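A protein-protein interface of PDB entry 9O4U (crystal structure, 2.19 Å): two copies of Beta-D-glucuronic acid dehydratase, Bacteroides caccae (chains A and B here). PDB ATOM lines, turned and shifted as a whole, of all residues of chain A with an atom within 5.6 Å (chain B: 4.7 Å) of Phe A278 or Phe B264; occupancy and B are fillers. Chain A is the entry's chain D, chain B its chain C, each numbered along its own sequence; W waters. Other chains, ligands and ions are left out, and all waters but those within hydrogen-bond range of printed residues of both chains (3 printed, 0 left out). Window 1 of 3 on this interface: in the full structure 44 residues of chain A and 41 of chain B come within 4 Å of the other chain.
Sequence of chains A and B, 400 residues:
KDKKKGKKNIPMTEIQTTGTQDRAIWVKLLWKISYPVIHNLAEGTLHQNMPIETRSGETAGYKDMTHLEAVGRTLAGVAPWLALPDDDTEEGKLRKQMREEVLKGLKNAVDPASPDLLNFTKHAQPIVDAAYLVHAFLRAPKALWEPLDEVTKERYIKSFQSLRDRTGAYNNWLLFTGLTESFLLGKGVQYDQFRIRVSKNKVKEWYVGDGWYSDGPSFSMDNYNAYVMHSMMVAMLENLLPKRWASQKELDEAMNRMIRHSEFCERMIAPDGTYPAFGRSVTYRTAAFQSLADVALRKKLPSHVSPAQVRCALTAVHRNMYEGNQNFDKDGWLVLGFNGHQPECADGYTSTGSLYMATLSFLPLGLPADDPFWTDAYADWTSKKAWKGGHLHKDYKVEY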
ATOM      1  N   TRP A 212      -1.295  24.250  -4.068  1.00  0.00           N
ATOM      2  CA  TRP A 212      -0.444  23.162  -4.524  1.00  0.00           C
ATOM      3  C   TRP A 212      -0.351  22.075  -3.466  1.00  0.00           C
ATOM      4  O   TRP A 212      -0.218  22.367  -2.276  1.00  0.00           O
ATOM      5  CB  TRP A 212       0.952  23.668  -4.852  1.00  0.00           C
ATOM      6  CG  TRP A 212       0.998  24.515  -6.042  1.00  0.00           C
ATOM      7  CD1 TRP A 212       0.670  25.835  -6.122  1.00  0.00           C
ATOM      8  CD2 TRP A 212       1.398  24.114  -7.357  1.00  0.00           C
ATOM      9  NE1 TRP A 212       0.846  26.283  -7.412  1.00  0.00           N
ATOM     10  CE2 TRP A 212       1.291  25.248  -8.191  1.00  0.00           C
ATOM     11  CE3 TRP A 212       1.851  22.908  -7.909  1.00  0.00           C
ATOM     12  CZ2 TRP A 212       1.608  25.212  -9.549  1.00  0.00           C
ATOM     13  CZ3 TRP A 212       2.158  22.870  -9.254  1.00  0.00           C
ATOM     14  CH2 TRP A 212       2.044  24.018 -10.059  1.00  0.00           C
ATOM     15  N   MET A 221       7.499  19.991  -8.773  1.00  0.00           N
ATOM     16  CA  MET A 221       7.070  21.125  -9.586  1.00  0.00           C
ATOM     17  C   MET A 221       6.804  20.595 -10.985  1.00  0.00           C
ATOM     18  O   MET A 221       7.674  20.598 -11.859  1.00  0.00           O
ATOM     19  CB  MET A 221       8.103  22.244  -9.561  1.00  0.00           C
ATOM     20  CG  MET A 221       7.718  23.537 -10.301  1.00  0.00           C
ATOM     21  SD  MET A 221       5.989  24.140 -10.357  1.00  0.00           S
ATOM     22  CE  MET A 221       5.330  23.823  -8.775  1.00  0.00           C
ATOM     23  N   ASP A 222       5.587  20.094 -11.180  1.00  0.00           N
ATOM     24  CA  ASP A 222       5.160  19.533 -12.453  1.00  0.00           C
ATOM     25  C   ASP A 222       3.654  19.725 -12.569  1.00  0.00           C
ATOM     26  O   ASP A 222       3.037  20.413 -11.749  1.00  0.00           O
ATOM     27  CB  ASP A 222       5.570  18.059 -12.568  1.00  0.00           C
ATOM     28  CG  ASP A 222       5.030  17.215 -11.450  1.00  0.00           C
ATOM     29  OD1 ASP A 222       3.853  17.386 -11.066  1.00  0.00           O
ATOM     30  OD2 ASP A 222       5.782  16.349 -10.959  1.00  0.00           O
ATOM     31  N   ASN A 223       3.054  19.081 -13.566  1.00  0.00           N
ATOM     32  CA  ASN A 223       1.645  19.264 -13.873  1.00  0.00           C
ATOM     33  C   ASN A 223       0.730  18.299 -13.135  1.00  0.00           C
ATOM     34  O   ASN A 223      -0.482  18.319 -13.381  1.00  0.00           O
ATOM     35  CB  ASN A 223       1.422  19.130 -15.381  1.00  0.00           C
ATOM     36  CG  ASN A 223       1.997  20.296 -16.146  1.00  0.00           C
ATOM     37  OD1 ASN A 223       1.855  21.453 -15.730  1.00  0.00           O
ATOM     38  ND2 ASN A 223       2.667  20.006 -17.256  1.00  0.00           N
ATOM     39  N   PHE A 264      -2.787  30.036 -11.480  1.00  0.00           N
ATOM     40  CA  PHE A 264      -1.438  29.873 -12.002  1.00  0.00           C
ATOM     41  C   PHE A 264      -1.460  29.266 -13.393  1.00  0.00           C
ATOM     42  O   PHE A 264      -0.717  29.703 -14.275  1.00  0.00           O
ATOM     43  CB  PHE A 264      -0.607  29.002 -11.067  1.00  0.00           C
ATOM     44  CG  PHE A 264       0.734  28.655 -11.628  1.00  0.00           C
ATOM     45  CD1 PHE A 264       1.784  29.556 -11.537  1.00  0.00           C
ATOM     46  CD2 PHE A 264       0.945  27.439 -12.260  1.00  0.00           C
ATOM     47  CE1 PHE A 264       3.027  29.257 -12.052  1.00  0.00           C
ATOM     48  CE2 PHE A 264       2.191  27.128 -12.787  1.00  0.00           C
ATOM     49  CZ  PHE A 264       3.239  28.035 -12.678  1.00  0.00           C
ATOM     50  N   MET A 268       0.095  30.845 -16.874  1.00  0.00           N
ATOM     51  CA  MET A 268       1.286  30.340 -17.551  1.00  0.00           C
ATOM     52  C   MET A 268       1.125  30.229 -19.063  1.00  0.00           C
ATOM     53  O   MET A 268       2.113  29.947 -19.753  1.00  0.00           O
ATOM     54  CB  MET A 268       1.721  28.987 -16.969  1.00  0.00           C
ATOM     55  CG  MET A 268       0.935  27.788 -17.434  1.00  0.00           C
ATOM     56  SD  MET A 268       1.730  26.274 -16.826  1.00  0.00           S
ATOM     57  CE  MET A 268       0.472  25.058 -17.243  1.00  0.00           C
ATOM     58  N   PRO A 276       4.761  26.485 -20.711  1.00  0.00           N
ATOM     59  CA  PRO A 276       6.072  25.865 -20.495  1.00  0.00           C
ATOM     60  C   PRO A 276       5.985  24.354 -20.535  1.00  0.00           C
ATOM     61  O   PRO A 276       4.998  23.761 -20.095  1.00  0.00           O
ATOM     62  CB  PRO A 276       6.484  26.349 -19.103  1.00  0.00           C
ATOM     63  CG  PRO A 276       5.612  27.556 -18.852  1.00  0.00           C
ATOM     64  CD  PRO A 276       4.326  27.257 -19.532  1.00  0.00           C
ATOM     65  N   ALA A 277       7.025  23.733 -21.067  1.00  0.00           N
ATOM     66  CA  ALA A 277       7.216  22.294 -20.913  1.00  0.00           C
ATOM     67  C   ALA A 277       8.097  22.089 -19.689  1.00  0.00           C
ATOM     68  O   ALA A 277       9.255  22.520 -19.676  1.00  0.00           O
ATOM     69  CB  ALA A 277       7.843  21.681 -22.164  1.00  0.00           C
ATOM     70  N   PHE A 278       7.538  21.468 -18.645  1.00  0.00           N
ATOM     71  CA  PHE A 278       8.286  21.233 -17.414  1.00  0.00           C
ATOM     72  C   PHE A 278       7.676  20.058 -16.661  1.00  0.00           C
ATOM     73  O   PHE A 278       6.479  19.789 -16.774  1.00  0.00           O
ATOM     74  CB  PHE A 278       8.294  22.477 -16.516  1.00  0.00           C
ATOM     75  CG  PHE A 278       6.965  22.768 -15.884  1.00  0.00           C
ATOM     76  CD1 PHE A 278       5.937  23.321 -16.632  1.00  0.00           C
ATOM     77  CD2 PHE A 278       6.744  22.479 -14.550  1.00  0.00           C
ATOM     78  CE1 PHE A 278       4.700  23.580 -16.057  1.00  0.00           C
ATOM     79  CE2 PHE A 278       5.503  22.739 -13.960  1.00  0.00           C
ATOM     80  CZ  PHE A 278       4.489  23.295 -14.722  1.00  0.00           C
ATOM     81  N   GLY A 279       8.509  19.373 -15.873  1.00  0.00           N
ATOM     82  CA  GLY A 279       8.039  18.277 -15.049  1.00  0.00           C
ATOM     83  C   GLY A 279       7.841  16.991 -15.828  1.00  0.00           C
ATOM     84  O   GLY A 279       7.984  16.925 -17.048  1.00  0.00           O
ATOM     85  N   ARG A 280       7.493  15.941 -15.098  1.00  0.00           N
ATOM     86  CA  ARG A 280       7.378  14.631 -15.725  1.00  0.00           C
ATOM     87  C   ARG A 280       6.042  14.490 -16.454  1.00  0.00           C
ATOM     88  O   ARG A 280       5.125  15.299 -16.299  1.00  0.00           O
ATOM     89  CB  ARG A 280       7.538  13.516 -14.692  1.00  0.00           C
ATOM     90  CG  ARG A 280       6.407  13.415 -13.670  1.00  0.00           C
ATOM     91  CD  ARG A 280       6.782  12.420 -12.568  1.00  0.00           C
ATOM     92  NE  ARG A 280       5.717  12.223 -11.593  1.00  0.00           N
ATOM     93  CZ  ARG A 280       4.788  11.274 -11.657  1.00  0.00           C
ATOM     94  NH1 ARG A 280       4.746  10.407 -12.659  1.00  0.00           N
ATOM     95  NH2 ARG A 280       3.876  11.195 -10.690  1.00  0.00           N
ATOM     96  N   VAL A 282       5.408  15.078 -19.452  1.00  0.00           N
ATOM     97  CA  VAL A 282       5.123  16.261 -20.251  1.00  0.00           C
ATOM     98  C   VAL A 282       4.289  15.887 -21.471  1.00  0.00           C
ATOM     99  O   VAL A 282       3.583  16.738 -22.022  1.00  0.00           O
ATOM    100  CB  VAL A 282       6.425  16.990 -20.639  1.00  0.00           C
ATOM    101  CG1 VAL A 282       7.032  16.407 -21.914  1.00  0.00           C
ATOM    102  CG2 VAL A 282       6.160  18.492 -20.795  1.00  0.00           C
ATOM    103  N   TRP B 212      12.404  23.731  -4.610  1.00  0.00           N
ATOM    104  CA  TRP B 212      11.594  24.835  -4.123  1.00  0.00           C
ATOM    105  C   TRP B 212      11.559  24.814  -2.606  1.00  0.00           C
ATOM    106  O   TRP B 212      11.503  23.743  -1.990  1.00  0.00           O
ATOM    107  CB  TRP B 212      10.166  24.777  -4.673  1.00  0.00           C
ATOM    108  CG  TRP B 212      10.058  25.044  -6.138  1.00  0.00           C
ATOM    109  CD1 TRP B 212      10.380  24.189  -7.151  1.00  0.00           C
ATOM    110  CD2 TRP B 212       9.562  26.237  -6.758  1.00  0.00           C
ATOM    111  NE1 TRP B 212      10.134  24.785  -8.365  1.00  0.00           N
ATOM    112  CE2 TRP B 212       9.630  26.042  -8.151  1.00  0.00           C
ATOM    113  CE3 TRP B 212       9.074  27.459  -6.269  1.00  0.00           C
ATOM    114  CZ2 TRP B 212       9.230  27.028  -9.068  1.00  0.00           C
ATOM    115  CZ3 TRP B 212       8.678  28.430  -7.176  1.00  0.00           C
ATOM    116  CH2 TRP B 212       8.757  28.209  -8.557  1.00  0.00           C
ATOM    117  N   ARG B 260      18.735  22.936  -9.498  1.00  0.00           N
ATOM    118  CA  ARG B 260      17.460  22.348  -9.903  1.00  0.00           C
ATOM    119  C   ARG B 260      16.428  23.431 -10.181  1.00  0.00           C
ATOM    120  O   ARG B 260      15.722  23.381 -11.196  1.00  0.00           O
ATOM    121  CB  ARG B 260      16.946  21.392  -8.828  1.00  0.00           C
ATOM    122  CG  ARG B 260      15.533  20.853  -9.119  1.00  0.00           C
ATOM    123  CD  ARG B 260      15.476  20.139 -10.464  1.00  0.00           C
ATOM    124  NE  ARG B 260      14.112  19.751 -10.795  1.00  0.00           N
ATOM    125  CZ  ARG B 260      13.688  19.450 -12.015  1.00  0.00           C
ATOM    126  NH1 ARG B 260      14.510  19.438 -13.051  1.00  0.00           N
ATOM    127  NH2 ARG B 260      12.401  19.176 -12.202  1.00  0.00           N
ATOM    128  N   HIS B 261      16.345  24.431  -9.300  1.00  0.00           N
ATOM    129  CA  HIS B 261      15.366  25.501  -9.463  1.00  0.00           C
ATOM    130  C   HIS B 261      15.594  26.293 -10.751  1.00  0.00           C
ATOM    131  O   HIS B 261      14.636  26.734 -11.393  1.00  0.00           O
ATOM    132  CB  HIS B 261      15.408  26.429  -8.247  1.00  0.00           C
ATOM    133  CG  HIS B 261      14.346  27.479  -8.263  1.00  0.00           C
ATOM    134  ND1 HIS B 261      14.578  28.757  -8.716  1.00  0.00           N
ATOM    135  CD2 HIS B 261      13.037  27.429  -7.918  1.00  0.00           C
ATOM    136  CE1 HIS B 261      13.456  29.455  -8.639  1.00  0.00           C
ATOM    137  NE2 HIS B 261      12.506  28.672  -8.162  1.00  0.00           N
ATOM    138  N   SER B 262      16.853  26.479 -11.157  1.00  0.00           N
ATOM    139  CA  SER B 262      17.097  27.246 -12.381  1.00  0.00           C
ATOM    140  C   SER B 262      16.538  26.545 -13.623  1.00  0.00           C
ATOM    141  O   SER B 262      16.207  27.215 -14.609  1.00  0.00           O
ATOM    142  CB  SER B 262      18.596  27.514 -12.554  1.00  0.00           C
ATOM    143  OG  SER B 262      19.287  26.316 -12.830  1.00  0.00           O
ATOM    144  N   GLU B 263      16.436  25.210 -13.595  1.00  0.00           N
ATOM    145  CA  GLU B 263      15.848  24.478 -14.711  1.00  0.00           C
ATOM    146  C   GLU B 263      14.424  24.940 -14.987  1.00  0.00           C
ATOM    147  O   GLU B 263      14.067  25.212 -16.140  1.00  0.00           O
ATOM    148  CB  GLU B 263      15.864  22.970 -14.438  1.00  0.00           C
ATOM    149  CG  GLU B 263      17.223  22.327 -14.465  1.00  0.00           C
ATOM    150  CD  GLU B 263      17.137  20.819 -14.590  1.00  0.00           C
ATOM    151  OE1 GLU B 263      16.911  20.322 -15.703  1.00  0.00           O
ATOM    152  OE2 GLU B 263      17.276  20.130 -13.573  1.00  0.00           O
ATOM    153  N   PHE B 264      13.587  25.004 -13.940  1.00  0.00           N
ATOM    154  CA  PHE B 264      12.221  25.490 -14.122  1.00  0.00           C
ATOM    155  C   PHE B 264      12.204  26.915 -14.662  1.00  0.00           C
ATOM    156  O   PHE B 264      11.405  27.241 -15.547  1.00  0.00           O
ATOM    157  CB  PHE B 264      11.432  25.436 -12.809  1.00  0.00           C
ATOM    158  CG  PHE B 264      10.072  26.121 -12.900  1.00  0.00           C
ATOM    159  CD1 PHE B 264       8.966  25.428 -13.369  1.00  0.00           C
ATOM    160  CD2 PHE B 264       9.919  27.461 -12.561  1.00  0.00           C
ATOM    161  CE1 PHE B 264       7.714  26.049 -13.473  1.00  0.00           C
ATOM    162  CE2 PHE B 264       8.681  28.089 -12.677  1.00  0.00           C
ATOM    163  CZ  PHE B 264       7.578  27.380 -13.129  1.00  0.00           C
ATOM    164  N   CYS B 265      13.044  27.788 -14.104  1.00  0.00           N
ATOM    165  CA  CYS B 265      13.064  29.173 -14.554  1.00  0.00           C
ATOM    166  C   CYS B 265      13.487  29.273 -16.015  1.00  0.00           C
ATOM    167  O   CYS B 265      12.910  30.056 -16.784  1.00  0.00           O
ATOM    168  CB  CYS B 265      13.985  29.989 -13.653  1.00  0.00           C
ATOM    169  SG  CYS B 265      13.431  30.003 -11.933  1.00  0.00           S
ATOM    170  N   GLU B 266      14.484  28.481 -16.425  1.00  0.00           N
ATOM    171  CA  GLU B 266      14.846  28.442 -17.840  1.00  0.00           C
ATOM    172  C   GLU B 266      13.714  27.870 -18.688  1.00  0.00           C
ATOM    173  O   GLU B 266      13.537  28.275 -19.837  1.00  0.00           O
ATOM    174  CB  GLU B 266      16.135  27.635 -18.047  1.00  0.00           C
ATOM    175  CG  GLU B 266      16.694  27.734 -19.461  1.00  0.00           C
ATOM    176  CD  GLU B 266      16.087  26.713 -20.418  1.00  0.00           C
ATOM    177  OE1 GLU B 266      15.493  25.736 -19.925  1.00  0.00           O
ATOM    178  OE2 GLU B 266      16.204  26.880 -21.654  1.00  0.00           O
ATOM    179  N   ARG B 267      12.921  26.952 -18.141  1.00  0.00           N
ATOM    180  CA  ARG B 267      11.855  26.367 -18.931  1.00  0.00           C
ATOM    181  C   ARG B 267      10.639  27.273 -19.061  1.00  0.00           C
ATOM    182  O   ARG B 267       9.842  27.075 -19.977  1.00  0.00           O
ATOM    183  CB  ARG B 267      11.438  25.025 -18.340  1.00  0.00           C
ATOM    184  CG  ARG B 267      12.328  23.872 -18.790  1.00  0.00           C
ATOM    185  CD  ARG B 267      12.125  22.660 -17.904  1.00  0.00           C
ATOM    186  NE  ARG B 267      12.988  21.537 -18.265  1.00  0.00           N
ATOM    187  CZ  ARG B 267      12.645  20.572 -19.111  1.00  0.00           C
ATOM    188  NH1 ARG B 267      11.481  20.584 -19.743  1.00  0.00           N
ATOM    189  NH2 ARG B 267      13.493  19.569 -19.328  1.00  0.00           N
ATOM    190  N   MET B 268      10.467  28.250 -18.182  1.00  0.00           N
ATOM    191  CA  MET B 268       9.289  29.095 -18.272  1.00  0.00           C
ATOM    192  C   MET B 268       9.465  30.268 -19.229  1.00  0.00           C
ATOM    193  O   MET B 268       8.515  31.029 -19.423  1.00  0.00           O
ATOM    194  CB  MET B 268       8.883  29.612 -16.885  1.00  0.00           C
ATOM    195  CG  MET B 268       9.716  30.741 -16.309  1.00  0.00           C
ATOM    196  SD  MET B 268       8.894  31.376 -14.811  1.00  0.00           S
ATOM    197  CE  MET B 268      10.238  32.226 -13.974  1.00  0.00           C
ATOM    198  N   ASP B 395      12.248  15.860 -18.477  1.00  0.00           N
ATOM    199  CA  ASP B 395      12.342  16.425 -17.139  1.00  0.00           C
ATOM    200  C   ASP B 395      11.725  15.469 -16.120  1.00  0.00           C
ATOM    201  O   ASP B 395      10.855  14.659 -16.455  1.00  0.00           O
ATOM    202  CB  ASP B 395      11.631  17.777 -17.093  1.00  0.00           C
ATOM    203  CG  ASP B 395      12.073  18.638 -15.926  1.00  0.00           C
ATOM    204  OD1 ASP B 395      13.055  18.292 -15.230  1.00  0.00           O
ATOM    205  OD2 ASP B 395      11.437  19.689 -15.719  1.00  0.00           O
HETATM  206  O   HOH W   1       9.645  24.869 -21.493  1.00  0.00           O
HETATM  207  O   HOH W   2       9.471  18.404 -11.828  1.00  0.00           O
HETATM  208  O   HOH W   3       9.360  16.149 -19.238  1.00  0.00           O
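Of the 11 printed residues of chain B, 4 touch a printed residue of chain A. Printed residues of chain B that touch a printed residue of chain A: Trp B212, Phe B264, Arg B267 and Asp B395. Among the printed residues, 8 pairs touch across the chains. Among the printed residues, no Asp or Glu carboxylate lies within 4 Å of a Lys or Arg side-chain nitrogen of the other chain.
Water W1 bridges O of Arg B267 (2.7 Å) and N of Ala A277 (2.9 Å). Water W3 bridges O of Gly A279 and N of Asp B395. Water W2 bridges O of Met A221 (2.8 Å) and NH2 of Arg B260 (3.1 Å).
Of the printed residues of chain B, Phe A278 touches Phe B264 and Asp B395. Printed residues of chain A within 4 Å of Phe B264: Met A221 and Phe A278. Printed residues of chain A within 4 Å of Trp B212: Met A221 (3.3 Å). Of the printed residues of chain A, Arg B267 touches Pro A276 (3.5 Å) and Ala A277 (3.0 Å). Of the printed residues of chain B, Met A221 touches Trp B212 (3.3 Å) and Phe B264 (3.8 Å). Of the printed residues of chain A, Asp B395 touches Phe A278, Gly A279 and Arg A280. Cys B265 touches none of the printed residues of chain A. The nearest residue of chain A that does not touch Phe B264 is Phe A264 (4.4 Å).
NH1 of Arg B267 lies within hydrogen-bond range of O of Ala A277 (3.0 Å). The side-chain carboxylate (OD2) of Asp B395 sits at hydrogen-bond distance from the backbone NH (N) of Gly A279 (2.9 Å).
Positions printed for both chains: 212, 264 and 268. Of the 8 pairs that touch across the chains among the printed residues, none has its exchanged pair printed and touching as well.
The side-chain carboxylate (OD1) of Asp B395 is in salt-bridge range of the guanidinium group (NH1) of Arg B260 (2.9 Å). The guanidinium group (NE) of Arg B267 is in salt-bridge range of the side-chain carboxylate (OD2) of Asp B395.
Among the printed residues, merely in contact across the chains: Met A221 with Trp B212, Met A221 with Phe B264, Pro A276 with Arg B267, Phe A278 with Phe B264, Phe A278 with Asp B395 and Arg A280 with Asp B395.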
